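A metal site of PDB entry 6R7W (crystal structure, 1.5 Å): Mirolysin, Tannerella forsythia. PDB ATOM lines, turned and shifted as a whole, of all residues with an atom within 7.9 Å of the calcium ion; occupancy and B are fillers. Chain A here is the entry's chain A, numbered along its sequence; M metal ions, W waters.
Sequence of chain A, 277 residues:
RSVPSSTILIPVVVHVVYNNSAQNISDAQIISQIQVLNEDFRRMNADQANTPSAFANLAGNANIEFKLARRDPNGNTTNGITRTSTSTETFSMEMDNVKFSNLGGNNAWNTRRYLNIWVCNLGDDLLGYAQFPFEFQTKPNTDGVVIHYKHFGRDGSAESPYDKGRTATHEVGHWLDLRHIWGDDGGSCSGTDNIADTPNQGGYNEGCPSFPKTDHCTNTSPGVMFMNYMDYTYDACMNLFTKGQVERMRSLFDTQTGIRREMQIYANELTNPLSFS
The calcium ion is bound by the side-chain carboxylate of Asp 193, the backbone carbonyl oxygen of Ile 195, water W1, the backbone carbonyl oxygen of Thr 198, water W2, water W4, water W3 and the side-chain hydroxyl of Thr 198.
Water W2 lies within hydrogen-bond range of O of Ile 181 (2.8 Å) and O of Pro 199 (2.8 Å). Water W4 lies within hydrogen-bond range of OG1 of Thr 192, N of Ile 195 and N of Asn 194.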
ATOM      1  N   HIS A 180     -16.157 -33.607  18.813  1.00  0.00           N
ATOM      2  CA  HIS A 180     -17.510 -33.138  19.147  1.00  0.00           C
ATOM      3  C   HIS A 180     -17.482 -32.251  20.364  1.00  0.00           C
ATOM      4  O   HIS A 180     -16.864 -32.585  21.381  1.00  0.00           O
ATOM      5  CB  HIS A 180     -18.416 -34.319  19.382  1.00  0.00           C
ATOM      6  CG  HIS A 180     -18.745 -34.989  18.097  1.00  0.00           C
ATOM      7  ND1 HIS A 180     -18.925 -36.352  18.028  1.00  0.00           N
ATOM      8  CD2 HIS A 180     -18.836 -34.469  16.853  1.00  0.00           C
ATOM      9  CE1 HIS A 180     -19.184 -36.618  16.763  1.00  0.00           C
ATOM     10  NE2 HIS A 180     -19.122 -35.519  16.005  1.00  0.00           N
ATOM     11  N   ILE A 181     -18.200 -31.129  20.271  1.00  0.00           N
ATOM     12  CA  ILE A 181     -18.169 -30.115  21.331  1.00  0.00           C
ATOM     13  C   ILE A 181     -18.684 -30.677  22.675  1.00  0.00           C
ATOM     14  O   ILE A 181     -18.217 -30.217  23.724  1.00  0.00           O
ATOM     15  CB  ILE A 181     -18.952 -28.864  20.838  1.00  0.00           C
ATOM     16  CG1 ILE A 181     -18.761 -27.706  21.807  1.00  0.00           C
ATOM     17  CG2 ILE A 181     -20.455 -29.130  20.534  1.00  0.00           C
ATOM     18  CD1 ILE A 181     -19.204 -26.362  21.186  1.00  0.00           C
ATOM     19  N   TRP A 182     -19.565 -31.675  22.647  1.00  0.00           N
ATOM     20  CA  TRP A 182     -20.118 -32.236  23.888  1.00  0.00           C
ATOM     21  C   TRP A 182     -19.195 -33.310  24.504  1.00  0.00           C
ATOM     22  O   TRP A 182     -19.474 -33.809  25.597  1.00  0.00           O
ATOM     23  CB  TRP A 182     -21.532 -32.786  23.679  1.00  0.00           C
ATOM     24  CG  TRP A 182     -21.594 -34.010  22.837  1.00  0.00           C
ATOM     25  CD1 TRP A 182     -21.611 -35.310  23.275  1.00  0.00           C
ATOM     26  CD2 TRP A 182     -21.693 -34.060  21.412  1.00  0.00           C
ATOM     27  NE1 TRP A 182     -21.662 -36.163  22.204  1.00  0.00           N
ATOM     28  CE2 TRP A 182     -21.706 -35.426  21.047  1.00  0.00           C
ATOM     29  CE3 TRP A 182     -21.774 -33.083  20.409  1.00  0.00           C
ATOM     30  CZ2 TRP A 182     -21.827 -35.838  19.711  1.00  0.00           C
ATOM     31  CZ3 TRP A 182     -21.885 -33.492  19.084  1.00  0.00           C
ATOM     32  CH2 TRP A 182     -21.917 -34.845  18.741  1.00  0.00           C
ATOM     33  N   GLY A 183     -18.121 -33.678  23.815  1.00  0.00           N
ATOM     34  CA  GLY A 183     -17.186 -34.635  24.414  1.00  0.00           C
ATOM     35  C   GLY A 183     -17.458 -36.120  24.269  1.00  0.00           C
ATOM     36  O   GLY A 183     -16.780 -36.913  24.932  1.00  0.00           O
ATOM     37  N   GLY A 191     -16.721 -35.792  29.821  1.00  0.00           N
ATOM     38  CA  GLY A 191     -15.979 -35.830  28.582  1.00  0.00           C
ATOM     39  C   GLY A 191     -15.589 -34.416  28.174  1.00  0.00           C
ATOM     40  O   GLY A 191     -16.071 -33.443  28.742  1.00  0.00           O
ATOM     41  N   THR A 192     -14.646 -34.318  27.249  1.00  0.00           N
ATOM     42  CA  THR A 192     -14.145 -33.021  26.826  1.00  0.00           C
ATOM     43  C   THR A 192     -13.846 -33.023  25.349  1.00  0.00           C
ATOM     44  O   THR A 192     -13.556 -34.062  24.769  1.00  0.00           O
ATOM     45  CB  THR A 192     -12.851 -32.688  27.637  1.00  0.00           C
ATOM     46  OG1 THR A 192     -12.397 -31.377  27.301  1.00  0.00           O
ATOM     47  CG2 THR A 192     -11.709 -33.705  27.425  1.00  0.00           C
ATOM     48  N   ASP A 193     -13.854 -31.819  24.749  1.00  0.00           N
ATOM     49  CA  ASP A 193     -13.393 -31.702  23.374  1.00  0.00           C
ATOM     50  C   ASP A 193     -11.973 -31.131  23.387  1.00  0.00           C
ATOM     51  O   ASP A 193     -11.384 -30.865  22.329  1.00  0.00           O
ATOM     52  CB  ASP A 193     -14.343 -30.843  22.497  1.00  0.00           C
ATOM     53  CG  ASP A 193     -14.480 -29.381  22.889  1.00  0.00           C
ATOM     54  OD1 ASP A 193     -14.107 -29.034  24.048  1.00  0.00           O
ATOM     55  OD2 ASP A 193     -14.950 -28.582  22.047  1.00  0.00           O
ATOM     56  N   ASN A 194     -11.383 -30.933  24.600  1.00  0.00           N
ATOM     57  CA  ASN A 194     -10.045 -30.365  24.804  1.00  0.00           C
ATOM     58  C   ASN A 194      -9.902 -28.988  24.152  1.00  0.00           C
ATOM     59  O   ASN A 194      -8.818 -28.617  23.700  1.00  0.00           O
ATOM     60  CB  ASN A 194      -8.952 -31.327  24.336  1.00  0.00           C
ATOM     61  CG  ASN A 194      -8.843 -32.526  25.263  1.00  0.00           C
ATOM     62  OD1 ASN A 194      -9.069 -33.668  24.866  1.00  0.00           O
ATOM     63  ND2 ASN A 194      -8.570 -32.278  26.550  1.00  0.00           N
ATOM     64  N   ILE A 195     -10.980 -28.188  24.178  1.00  0.00           N
ATOM     65  CA  ILE A 195     -11.001 -26.785  23.753  1.00  0.00           C
ATOM     66  C   ILE A 195     -11.598 -25.984  24.896  1.00  0.00           C
ATOM     67  O   ILE A 195     -12.785 -26.139  25.249  1.00  0.00           O
ATOM     68  CB  ILE A 195     -11.781 -26.559  22.447  1.00  0.00           C
ATOM     69  CG1 ILE A 195     -11.324 -27.476  21.300  1.00  0.00           C
ATOM     70  CG2 ILE A 195     -11.732 -25.091  22.067  1.00  0.00           C
ATOM     71  CD1 ILE A 195      -9.908 -27.169  20.773  1.00  0.00           C
ATOM     72  N   ALA A 196     -10.790 -25.102  25.491  1.00  0.00           N
ATOM     73  CA  ALA A 196     -11.238 -24.365  26.655  1.00  0.00           C
ATOM     74  C   ALA A 196     -12.337 -23.356  26.364  1.00  0.00           C
ATOM     75  O   ALA A 196     -13.209 -23.172  27.218  1.00  0.00           O
ATOM     76  CB  ALA A 196     -10.058 -23.664  27.293  1.00  0.00           C
ATOM     77  N   ASP A 197     -12.365 -22.738  25.160  1.00  0.00           N
ATOM     78  CA  ASP A 197     -13.363 -21.714  24.870  1.00  0.00           C
ATOM     79  C   ASP A 197     -14.674 -22.262  24.305  1.00  0.00           C
ATOM     80  O   ASP A 197     -15.598 -21.473  24.069  1.00  0.00           O
ATOM     81  CB  ASP A 197     -12.813 -20.594  23.989  1.00  0.00           C
ATOM     82  CG  ASP A 197     -12.461 -20.983  22.592  1.00  0.00           C
ATOM     83  OD1 ASP A 197     -12.699 -22.150  22.232  1.00  0.00           O
ATOM     84  OD2 ASP A 197     -11.956 -20.113  21.846  1.00  0.00           O
ATOM     85  N   THR A 198     -14.798 -23.605  24.208  1.00  0.00           N
ATOM     86  CA  THR A 198     -16.123 -24.184  23.927  1.00  0.00           C
ATOM     87  C   THR A 198     -16.681 -24.557  25.301  1.00  0.00           C
ATOM     88  O   THR A 198     -16.077 -25.363  26.024  1.00  0.00           O
ATOM     89  CB  THR A 198     -16.073 -25.380  22.976  1.00  0.00           C
ATOM     90  OG1 THR A 198     -15.102 -26.330  23.443  1.00  0.00           O
ATOM     91  CG2 THR A 198     -15.780 -24.953  21.551  1.00  0.00           C
ATOM     92  N   PRO A 199     -17.819 -23.986  25.703  1.00  0.00           N
ATOM     93  CA  PRO A 199     -18.378 -24.295  27.039  1.00  0.00           C
ATOM     94  C   PRO A 199     -18.618 -25.795  27.230  1.00  0.00           C
ATOM     95  O   PRO A 199     -19.066 -26.476  26.289  1.00  0.00           O
ATOM     96  CB  PRO A 199     -19.688 -23.512  27.064  1.00  0.00           C
ATOM     97  CG  PRO A 199     -19.545 -22.423  26.041  1.00  0.00           C
ATOM     98  CD  PRO A 199     -18.643 -22.996  24.966  1.00  0.00           C
ATOM     99  N   ASN A 200     -18.377 -26.294  28.432  1.00  0.00           N
ATOM    100  CA  ASN A 200     -18.651 -27.708  28.705  1.00  0.00           C
ATOM    101  C   ASN A 200     -20.133 -27.977  28.394  1.00  0.00           C
ATOM    102  O   ASN A 200     -21.003 -27.169  28.708  1.00  0.00           O
ATOM    103  CB  ASN A 200     -18.319 -28.035  30.143  1.00  0.00           C
ATOM    104  CG  ASN A 200     -18.265 -29.518  30.386  1.00  0.00           C
ATOM    105  OD1 ASN A 200     -18.255 -30.316  29.449  1.00  0.00           O
ATOM    106  ND2 ASN A 200     -18.236 -29.916  31.669  1.00  0.00           N
ATOM    107  N   GLN A 201     -20.397 -29.084  27.718  1.00  0.00           N
ATOM    108  CA  GLN A 201     -21.738 -29.379  27.209  1.00  0.00           C
ATOM    109  C   GLN A 201     -22.048 -30.824  27.467  1.00  0.00           C
ATOM    110  O   GLN A 201     -21.169 -31.683  27.365  1.00  0.00           O
ATOM    111  CB  GLN A 201     -21.715 -29.053  25.697  1.00  0.00           C
ATOM    112  CG  GLN A 201     -23.019 -29.307  24.948  1.00  0.00           C
ATOM    113  CD  GLN A 201     -22.891 -28.872  23.503  1.00  0.00           C
ATOM    114  OE1 GLN A 201     -22.299 -27.851  23.189  1.00  0.00           O
ATOM    115  NE2 GLN A 201     -23.471 -29.628  22.587  1.00  0.00           N
ATOM    116  N   GLN A 245     -10.600 -23.651  18.714  1.00  0.00           N
ATOM    117  CA  GLN A 245     -10.648 -24.697  17.690  1.00  0.00           C
ATOM    118  C   GLN A 245      -9.700 -24.351  16.549  1.00  0.00           C
ATOM    119  O   GLN A 245      -8.994 -25.245  16.047  1.00  0.00           O
ATOM    120  CB  GLN A 245     -12.075 -24.849  17.157  1.00  0.00           C
ATOM    121  CG  GLN A 245     -12.996 -25.509  18.203  1.00  0.00           C
ATOM    122  CD  GLN A 245     -14.408 -25.528  17.705  1.00  0.00           C
ATOM    123  OE1 GLN A 245     -14.891 -24.538  17.158  1.00  0.00           O
ATOM    124  NE2 GLN A 245     -15.110 -26.644  17.903  1.00  0.00           N
HETATM  125 CA    CA M   1     -14.766 -27.428  25.704  1.00  0.00          CA
HETATM  126  O   HOH W   1     -14.871 -26.855  28.071  1.00  0.00           O
HETATM  127  O   HOH W   2     -17.078 -28.028  25.001  1.00  0.00           O
HETATM  128  O   HOH W   3     -15.392 -29.622  26.803  1.00  0.00           O
HETATM  129  O   HOH W   4     -12.755 -28.613  26.642  1.00  0.00           O
